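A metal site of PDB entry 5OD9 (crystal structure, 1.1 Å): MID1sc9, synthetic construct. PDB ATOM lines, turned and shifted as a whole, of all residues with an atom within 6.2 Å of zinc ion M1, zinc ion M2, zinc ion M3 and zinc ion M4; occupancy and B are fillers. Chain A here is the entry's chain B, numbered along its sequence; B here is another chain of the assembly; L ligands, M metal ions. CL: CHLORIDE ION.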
ATOM      1  N   GLN A  33     -20.168  -7.220 -16.639  1.00  0.00           N
ATOM      2  CA  GLN A  33     -19.382  -6.272 -15.898  1.00  0.00           C
ATOM      3  C   GLN A  33     -19.960  -6.046 -14.517  1.00  0.00           C
ATOM      4  O   GLN A  33     -19.272  -5.888 -13.512  1.00  0.00           O
ATOM      5  CB  GLN A  33     -19.390  -4.929 -16.653  1.00  0.00           C
ATOM      6  CG  GLN A  33     -18.472  -4.945 -17.871  1.00  0.00           C
ATOM      7  CD  GLN A  33     -18.531  -3.672 -18.701  1.00  0.00           C
ATOM      8  OE1 GLN A  33     -19.372  -2.777 -18.446  1.00  0.00           O
ATOM      9  NE2 GLN A  33     -17.606  -3.660 -19.663  1.00  0.00           N
ATOM     10  N   GLU A  34     -21.292  -6.018 -14.453  1.00  0.00           N
ATOM     11  CA  GLU A  34     -22.008  -5.857 -13.176  1.00  0.00           C
ATOM     12  C   GLU A  34     -21.963  -7.118 -12.345  1.00  0.00           C
ATOM     13  O   GLU A  34     -21.823  -7.016 -11.135  1.00  0.00           O
ATOM     14  CB  GLU A  34     -23.410  -5.321 -13.414  1.00  0.00           C
ATOM     15  CG  GLU A  34     -23.367  -3.806 -13.528  1.00  0.00           C
ATOM     16  CD  GLU A  34     -23.288  -3.139 -12.184  1.00  0.00           C
ATOM     17  OE1 GLU A  34     -22.169  -3.202 -11.582  1.00  0.00           O
ATOM     18  OE2 GLU A  34     -24.348  -2.648 -11.745  1.00  0.00           O
ATOM     19  N   HIS A  37     -18.720  -7.017 -10.327  1.00  0.00           N
ATOM     20  CA  HIS A  37     -18.593  -6.128  -9.175  1.00  0.00           C
ATOM     21  C   HIS A  37     -18.727  -6.895  -7.887  1.00  0.00           C
ATOM     22  O   HIS A  37     -17.754  -6.831  -7.104  1.00  0.00           O
ATOM     23  CB  HIS A  37     -19.563  -4.972  -9.482  1.00  0.00           C
ATOM     24  CG  HIS A  37     -19.746  -3.986  -8.387  1.00  0.00           C
ATOM     25  ND1 HIS A  37     -20.649  -2.982  -8.530  1.00  0.00           N
ATOM     26  CD2 HIS A  37     -19.184  -3.818  -7.174  1.00  0.00           C
ATOM     27  CE1 HIS A  37     -20.577  -2.255  -7.408  1.00  0.00           C
ATOM     28  NE2 HIS A  37     -19.708  -2.744  -6.539  1.00  0.00           N
ATOM     29  N   PRO A  38     -19.852  -7.496  -7.534  1.00  0.00           N
ATOM     30  CA  PRO A  38     -19.847  -8.219  -6.252  1.00  0.00           C
ATOM     31  C   PRO A  38     -18.807  -9.326  -6.202  1.00  0.00           C
ATOM     32  O   PRO A  38     -18.303  -9.629  -5.139  1.00  0.00           O
ATOM     33  CB  PRO A  38     -21.249  -8.792  -6.102  1.00  0.00           C
ATOM     34  CG  PRO A  38     -22.057  -8.224  -7.202  1.00  0.00           C
ATOM     35  CD  PRO A  38     -21.160  -7.524  -8.150  1.00  0.00           C
ATOM     36  N   HIS A  41     -15.596  -7.848  -5.076  1.00  0.00           N
ATOM     37  CA  HIS A  41     -15.574  -7.555  -3.654  1.00  0.00           C
ATOM     38  C   HIS A  41     -15.386  -8.807  -2.815  1.00  0.00           C
ATOM     39  O   HIS A  41     -14.672  -8.754  -1.817  1.00  0.00           O
ATOM     40  CB  HIS A  41     -16.879  -6.887  -3.212  1.00  0.00           C
ATOM     41  CG  HIS A  41     -17.104  -5.480  -3.577  1.00  0.00           C
ATOM     42  ND1 HIS A  41     -16.147  -4.493  -3.649  1.00  0.00           N
ATOM     43  CD2 HIS A  41     -18.264  -4.832  -3.882  1.00  0.00           C
ATOM     44  CE1 HIS A  41     -16.688  -3.364  -3.942  1.00  0.00           C
ATOM     45  NE2 HIS A  41     -18.004  -3.515  -4.092  1.00  0.00           N
ATOM     46  N   HIS A  63     -14.654  -0.010  -8.265  1.00  0.00           N
ATOM     47  CA  HIS A  63     -16.043  -0.437  -8.061  1.00  0.00           C
ATOM     48  C   HIS A  63     -16.823   0.486  -7.152  1.00  0.00           C
ATOM     49  O   HIS A  63     -17.969   0.794  -7.461  1.00  0.00           O
ATOM     50  CB  HIS A  63     -16.088  -1.866  -7.550  1.00  0.00           C
ATOM     51  CG  HIS A  63     -15.665  -2.838  -8.607  1.00  0.00           C
ATOM     52  ND1 HIS A  63     -16.416  -3.203  -9.668  1.00  0.00           N
ATOM     53  CD2 HIS A  63     -14.482  -3.464  -8.713  1.00  0.00           C
ATOM     54  CE1 HIS A  63     -15.731  -4.062 -10.427  1.00  0.00           C
ATOM     55  NE2 HIS A  63     -14.522  -4.254  -9.884  1.00  0.00           N
ATOM     56  N   VAL A  64     -16.233   0.944  -6.071  1.00  0.00           N
ATOM     57  CA  VAL A  64     -16.882   1.930  -5.177  1.00  0.00           C
ATOM     58  C   VAL A  64     -17.332   3.149  -5.977  1.00  0.00           C
ATOM     59  O   VAL A  64     -18.442   3.639  -5.832  1.00  0.00           O
ATOM     60  CB  VAL A  64     -15.985   2.307  -3.973  1.00  0.00           C
ATOM     61  CG1 VAL A  64     -16.553   3.485  -3.228  1.00  0.00           C
ATOM     62  CG2 VAL A  64     -15.750   1.122  -3.072  1.00  0.00           C
ATOM     63  N   ILE A  66     -17.640   3.487  -9.353  1.00  0.00           N
ATOM     64  CA  ILE A  66     -18.675   3.131 -10.347  1.00  0.00           C
ATOM     65  C   ILE A  66     -20.034   3.177  -9.668  1.00  0.00           C
ATOM     66  O   ILE A  66     -20.983   3.734 -10.219  1.00  0.00           O
ATOM     67  CB  ILE A  66     -18.410   1.805 -10.977  1.00  0.00           C
ATOM     68  CG1 ILE A  66     -17.140   1.787 -11.854  1.00  0.00           C
ATOM     69  CG2 ILE A  66     -19.612   1.316 -11.771  1.00  0.00           C
ATOM     70  CD1 ILE A  66     -16.582   0.436 -12.113  1.00  0.00           C
ATOM     71  N   HIS A  67     -20.139   2.571  -8.485  1.00  0.00           N
ATOM     72  CA  HIS A  67     -21.431   2.500  -7.830  1.00  0.00           C
ATOM     73  C   HIS A  67     -21.957   3.904  -7.472  1.00  0.00           C
ATOM     74  O   HIS A  67     -23.138   4.212  -7.695  1.00  0.00           O
ATOM     75  CB  HIS A  67     -21.315   1.614  -6.575  1.00  0.00           C
ATOM     76  CG  HIS A  67     -22.654   1.118  -6.099  1.00  0.00           C
ATOM     77  ND1 HIS A  67     -22.768   0.170  -5.109  1.00  0.00           N
ATOM     78  CD2 HIS A  67     -23.909   1.343  -6.500  1.00  0.00           C
ATOM     79  CE1 HIS A  67     -24.038  -0.134  -4.937  1.00  0.00           C
ATOM     80  NE2 HIS A  67     -24.766   0.551  -5.785  1.00  0.00           N
ATOM     81  N   ARG A  70     -23.164   5.585 -10.570  1.00  0.00           N
ATOM     82  CA  ARG A  70     -24.443   5.092 -11.032  1.00  0.00           C
ATOM     83  C   ARG A  70     -25.606   5.623 -10.202  1.00  0.00           C
ATOM     84  O   ARG A  70     -26.636   5.990 -10.694  1.00  0.00           O
ATOM     85  CB  ARG A  70     -24.385   3.550 -11.085  1.00  0.00           C
ATOM     86  CG  ARG A  70     -25.462   3.003 -12.002  1.00  0.00           C
ATOM     87  CD  ARG A  70     -25.531   1.477 -11.907  1.00  0.00           C
ATOM     88  NE  ARG A  70     -24.231   0.833 -12.037  1.00  0.00           N
ATOM     89  CZ  ARG A  70     -23.650   0.439 -13.163  1.00  0.00           C
ATOM     90  NH1 ARG A  70     -24.224   0.613 -14.305  1.00  0.00           N
ATOM     91  NH2 ARG A  70     -22.458  -0.142 -13.055  1.00  0.00           N
ATOM     92  N   ALA A  71     -25.376   5.699  -8.884  1.00  0.00           N
ATOM     93  CA  ALA A  71     -26.426   6.164  -7.975  1.00  0.00           C
ATOM     94  C   ALA A  71     -26.779   7.627  -8.284  1.00  0.00           C
ATOM     95  O   ALA A  71     -27.906   8.030  -8.070  1.00  0.00           O
ATOM     96  CB  ALA A  71     -25.982   6.043  -6.511  1.00  0.00           C
ATOM     97  N   GLN B  33     -28.862 -10.659  -2.844  1.00  0.00           N
ATOM     98  CA  GLN B  33     -28.602  -9.261  -3.238  1.00  0.00           C
ATOM     99  C   GLN B  33     -27.692  -9.183  -4.468  1.00  0.00           C
ATOM    100  O   GLN B  33     -27.914  -8.375  -5.372  1.00  0.00           O
ATOM    101  CB  GLN B  33     -28.031  -8.527  -2.062  1.00  0.00           C
ATOM    102  CG  GLN B  33     -29.063  -8.274  -0.923  1.00  0.00           C
ATOM    103  CD  GLN B  33     -28.461  -7.559   0.264  1.00  0.00           C
ATOM    104  OE1 GLN B  33     -27.262  -7.743   0.537  1.00  0.00           O
ATOM    105  NE2 GLN B  33     -29.247  -6.842   1.031  1.00  0.00           N
ATOM    106  N   GLU B  34     -26.659 -10.016  -4.476  1.00  0.00           N
ATOM    107  CA  GLU B  34     -25.701  -9.935  -5.570  1.00  0.00           C
ATOM    108  C   GLU B  34     -26.322 -10.409  -6.872  1.00  0.00           C
ATOM    109  O   GLU B  34     -25.981  -9.870  -7.936  1.00  0.00           O
ATOM    110  CB  GLU B  34     -24.450 -10.742  -5.159  1.00  0.00           C
ATOM    111  CG  GLU B  34     -23.720 -10.009  -4.030  1.00  0.00           C
ATOM    112  CD  GLU B  34     -22.518 -10.732  -3.479  1.00  0.00           C
ATOM    113  OE1 GLU B  34     -22.362 -11.917  -3.724  1.00  0.00           O
ATOM    114  OE2 GLU B  34     -21.793 -10.030  -2.756  1.00  0.00           O
ATOM    115  N   HIS B  37     -28.275  -7.316  -7.950  1.00  0.00           N
ATOM    116  CA  HIS B  37     -27.466  -6.108  -8.268  1.00  0.00           C
ATOM    117  C   HIS B  37     -27.548  -5.639  -9.712  1.00  0.00           C
ATOM    118  O   HIS B  37     -27.940  -4.467  -9.923  1.00  0.00           O
ATOM    119  CB  HIS B  37     -26.036  -6.363  -7.769  1.00  0.00           C
ATOM    120  CG  HIS B  37     -25.070  -5.258  -7.938  1.00  0.00           C
ATOM    121  ND1 HIS B  37     -24.606  -4.503  -6.863  1.00  0.00           N
ATOM    122  CD2 HIS B  37     -24.468  -4.739  -9.053  1.00  0.00           C
ATOM    123  CE1 HIS B  37     -23.766  -3.624  -7.374  1.00  0.00           C
ATOM    124  NE2 HIS B  37     -23.641  -3.695  -8.707  1.00  0.00           N
ATOM    125  N   TRP B  40     -31.434  -4.609 -10.523  1.00  0.00           N
ATOM    126  CA  TRP B  40     -31.821  -3.345  -9.911  1.00  0.00           C
ATOM    127  C   TRP B  40     -31.119  -2.167 -10.553  1.00  0.00           C
ATOM    128  O   TRP B  40     -31.743  -1.135 -10.815  1.00  0.00           O
ATOM    129  CB  TRP B  40     -31.512  -3.391  -8.402  1.00  0.00           C
ATOM    130  CG  TRP B  40     -31.611  -2.043  -7.781  1.00  0.00           C
ATOM    131  CD1 TRP B  40     -30.555  -1.329  -7.257  1.00  0.00           C
ATOM    132  CD2 TRP B  40     -32.754  -1.215  -7.595  1.00  0.00           C
ATOM    133  NE1 TRP B  40     -30.972  -0.130  -6.780  1.00  0.00           N
ATOM    134  CE2 TRP B  40     -32.327  -0.030  -6.974  1.00  0.00           C
ATOM    135  CE3 TRP B  40     -34.143  -1.350  -7.908  1.00  0.00           C
ATOM    136  CZ2 TRP B  40     -33.192   0.992  -6.657  1.00  0.00           C
ATOM    137  CZ3 TRP B  40     -34.995  -0.330  -7.587  1.00  0.00           C
ATOM    138  CH2 TRP B  40     -34.505   0.806  -6.981  1.00  0.00           C
ATOM    139  N   HIS B  41     -29.844  -2.284 -10.875  1.00  0.00           N
ATOM    140  CA  HIS B  41     -29.200  -1.140 -11.523  1.00  0.00           C
ATOM    141  C   HIS B  41     -29.726  -0.864 -12.913  1.00  0.00           C
ATOM    142  O   HIS B  41     -29.924   0.291 -13.268  1.00  0.00           O
ATOM    143  CB  HIS B  41     -27.694  -1.376 -11.532  1.00  0.00           C
ATOM    144  CG  HIS B  41     -27.103  -0.997 -10.200  1.00  0.00           C
ATOM    145  ND1 HIS B  41     -25.802  -1.312  -9.861  1.00  0.00           N
ATOM    146  CD2 HIS B  41     -27.619  -0.301  -9.153  1.00  0.00           C
ATOM    147  CE1 HIS B  41     -25.585  -0.834  -8.643  1.00  0.00           C
ATOM    148  NE2 HIS B  41     -26.628  -0.219  -8.154  1.00  0.00           N
ATOM    149  N   GLU B  60     -31.543   3.326  -3.456  1.00  0.00           N
ATOM    150  CA  GLU B  60     -30.232   3.159  -4.086  1.00  0.00           C
ATOM    151  C   GLU B  60     -29.098   3.603  -3.178  1.00  0.00           C
ATOM    152  O   GLU B  60     -28.039   2.958  -3.123  1.00  0.00           O
ATOM    153  CB  GLU B  60     -30.230   3.850  -5.461  1.00  0.00           C
ATOM    154  CG  GLU B  60     -28.884   3.885  -6.116  1.00  0.00           C
ATOM    155  CD  GLU B  60     -28.135   2.550  -6.254  1.00  0.00           C
ATOM    156  OE1 GLU B  60     -28.766   1.506  -6.266  1.00  0.00           O
ATOM    157  OE2 GLU B  60     -26.906   2.567  -6.298  1.00  0.00           O
ATOM    158  N   HIS B  63     -28.383   0.766  -0.953  1.00  0.00           N
ATOM    159  CA  HIS B  63     -27.581  -0.197  -1.648  1.00  0.00           C
ATOM    160  C   HIS B  63     -26.095   0.174  -1.651  1.00  0.00           C
ATOM    161  O   HIS B  63     -25.272  -0.673  -1.368  1.00  0.00           O
ATOM    162  CB  HIS B  63     -28.132  -0.310  -3.096  1.00  0.00           C
ATOM    163  CG  HIS B  63     -27.427  -1.397  -3.879  1.00  0.00           C
ATOM    164  ND1 HIS B  63     -27.176  -1.188  -5.259  1.00  0.00           N
ATOM    165  CD2 HIS B  63     -26.992  -2.623  -3.556  1.00  0.00           C
ATOM    166  CE1 HIS B  63     -26.600  -2.334  -5.651  1.00  0.00           C
ATOM    167  NE2 HIS B  63     -26.462  -3.235  -4.686  1.00  0.00           N
ATOM    168  N   VAL B  64     -25.805   1.422  -1.953  1.00  0.00           N
ATOM    169  CA  VAL B  64     -24.410   1.880  -1.872  1.00  0.00           C
ATOM    170  C   VAL B  64     -23.880   1.636  -0.475  1.00  0.00           C
ATOM    171  O   VAL B  64     -22.720   1.139  -0.332  1.00  0.00           O
ATOM    172  CB  VAL B  64     -24.362   3.382  -2.226  1.00  0.00           C
ATOM    173  CG1 VAL B  64     -23.027   3.984  -1.865  1.00  0.00           C
ATOM    174  CG2 VAL B  64     -24.687   3.605  -3.709  1.00  0.00           C
ATOM    175  N   HIS B  67     -23.049  -1.999   0.302  1.00  0.00           N
ATOM    176  CA  HIS B  67     -21.761  -2.387  -0.190  1.00  0.00           C
ATOM    177  C   HIS B  67     -20.658  -1.921   0.737  1.00  0.00           C
ATOM    178  O   HIS B  67     -19.719  -2.646   1.041  1.00  0.00           O
ATOM    179  CB  HIS B  67     -21.494  -1.817  -1.594  1.00  0.00           C
ATOM    180  CG  HIS B  67     -22.047  -2.611  -2.702  1.00  0.00           C
ATOM    181  ND1 HIS B  67     -21.298  -3.073  -3.779  1.00  0.00           N
ATOM    182  CD2 HIS B  67     -23.290  -3.100  -2.873  1.00  0.00           C
ATOM    183  CE1 HIS B  67     -22.115  -3.780  -4.549  1.00  0.00           C
ATOM    184  NE2 HIS B  67     -23.347  -3.836  -4.051  1.00  0.00           N
ATOM    185  N   GLN B  68     -20.768  -0.717   1.250  1.00  0.00           N
ATOM    186  CA  GLN B  68     -19.716  -0.185   2.117  1.00  0.00           C
ATOM    187  C   GLN B  68     -19.664  -0.923   3.456  1.00  0.00           C
ATOM    188  O   GLN B  68     -18.592  -1.227   3.929  1.00  0.00           O
ATOM    189  CB  GLN B  68     -19.858   1.323   2.338  1.00  0.00           C
ATOM    190  CG  GLN B  68     -19.633   2.052   1.002  1.00  0.00           C
ATOM    191  CD  GLN B  68     -18.230   2.356   0.557  1.00  0.00           C
ATOM    192  OE1 GLN B  68     -17.366   2.821   1.306  1.00  0.00           O
ATOM    193  NE2 GLN B  68     -17.886   2.152  -0.722  1.00  0.00           N
ATOM    194  N   ARG B  70     -20.705  -4.005   4.009  1.00  0.00           N
ATOM    195  CA  ARG B  70     -20.242  -5.383   3.770  1.00  0.00           C
ATOM    196  C   ARG B  70     -18.722  -5.334   3.617  1.00  0.00           C
ATOM    197  O   ARG B  70     -18.069  -6.236   4.181  1.00  0.00           O
ATOM    198  CB  ARG B  70     -20.985  -6.003   2.567  1.00  0.00           C
ATOM    199  CG  ARG B  70     -20.453  -7.235   1.897  1.00  0.00           C
ATOM    200  CD  ARG B  70     -21.572  -7.845   0.999  1.00  0.00           C
ATOM    201  NE  ARG B  70     -22.760  -8.292   1.722  1.00  0.00           N
ATOM    202  CZ  ARG B  70     -24.015  -8.046   1.429  1.00  0.00           C
ATOM    203  NH1 ARG B  70     -24.302  -7.319   0.343  1.00  0.00           N
ATOM    204  NH2 ARG B  70     -25.019  -8.523   2.216  1.00  0.00           N
HETATM  205 CL    CL L   1     -22.386  -0.407  -9.580  1.00  0.00          CL
HETATM  206 CL    CL L   2     -25.422  -6.592  -4.002  1.00  0.00          CL
HETATM  207 CL    CL L   3     -19.571  -0.213  -4.019  1.00  0.00          CL
HETATM  208 ZN    ZN M   1     -22.249  -2.666  -9.709  1.00  0.00          ZN
HETATM  209 ZN    ZN M   2     -25.007  -4.611  -4.903  1.00  0.00          ZN
HETATM  210 ZN    ZN M   3     -19.584  -2.357  -4.574  1.00  0.00          ZN
HETATM  211 ZN    ZN M   4     -26.769   0.469  -6.274  1.00  0.00          ZN
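The side-chain carboxylate (OE2) of Glu 34 of chain A lies within hydrogen-bond range of a ring nitrogen (ND1) of His 41 of chain B (2.7 Å). A ring nitrogen (ND1) of His 41 of chain B sits close to a ring nitrogen (NE2) of His 37 of chain B, at 3.4 Å. The guanidinium group (NE) of Arg 70 of chain A sits at hydrogen-bond distance from a ring nitrogen (ND1) of His 41 of chain B (3.4 Å). OE2 of Glu 34 of chain A lies within salt-bridge range of NH2 of Arg 70 of chain A. The side-chain carboxylate (OE1) of Glu 60 of chain B sits close to the indole nitrogen (NE1) of Trp 40 of chain B (2.8 Å).
The nearest printed residue that does not touch zinc ion M1 is Arg 70 of chain A (4.2 Å).
Within 4 Å of zinc ion M2: His 37 of chain B, His 63 of chain B and His 67 of chain B. The nearest printed residue that does not touch zinc ion M2 is His 67 of chain A (4.6 Å).
Three residues have an atom within 4 Å of zinc ion M3: His 37 of chain A, His 41 of chain A and His 67 of chain B.
Within 4 Å of zinc ion M4: His 67 of chain A, His 41 of chain B, Glu 60 of chain B and His 63 of chain B. The nearest printed residue that does not touch zinc ion M4 is Trp 40 of chain B (4.3 Å).
OE1 of Glu 34 of chain A is bound to zinc ion M1 (1.9 Å). NE2 of His 37 of chain B binds zinc ion M1 (2.0 Å). Zinc ion M1 is bound by a ring nitrogen (ND1) of His 37 of chain A (2.0 Å). CL of CL L1 binds zinc ion M1 (2.3 Å).
Zinc ion M2 is bound by a ring nitrogen (ND1) of His 37 of chain B (2.0 Å), a ring nitrogen (NE2) of His 63 of chain B (2.0 Å), a ring nitrogen (NE2) of His 67 of chain B (2.0 Å) and a chlorine (CL) of CL L2 (2.2 Å).
NE2 of His 37 of chain A binds zinc ion M3 (2.0 Å). NE2 of His 41 of chain A is bound to zinc ion M3. A ring nitrogen (ND1) of His 67 of chain B is bound to zinc ion M3, 2.0 Å away. Zinc ion M3 is bound by a chlorine (CL) of CL L3 (2.2 Å). Zinc ion M3 has four donor atoms within binding distance.
Zinc ion M4 is bound by ND1 of His 63 of chain B, NE2 of His 41 of chain B, NE2 of His 67 of chain A, OE2 of Glu 60 of chain B and OE1 of Glu 60 of chain B. Zinc ion M4 has five donor atoms within binding distance.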
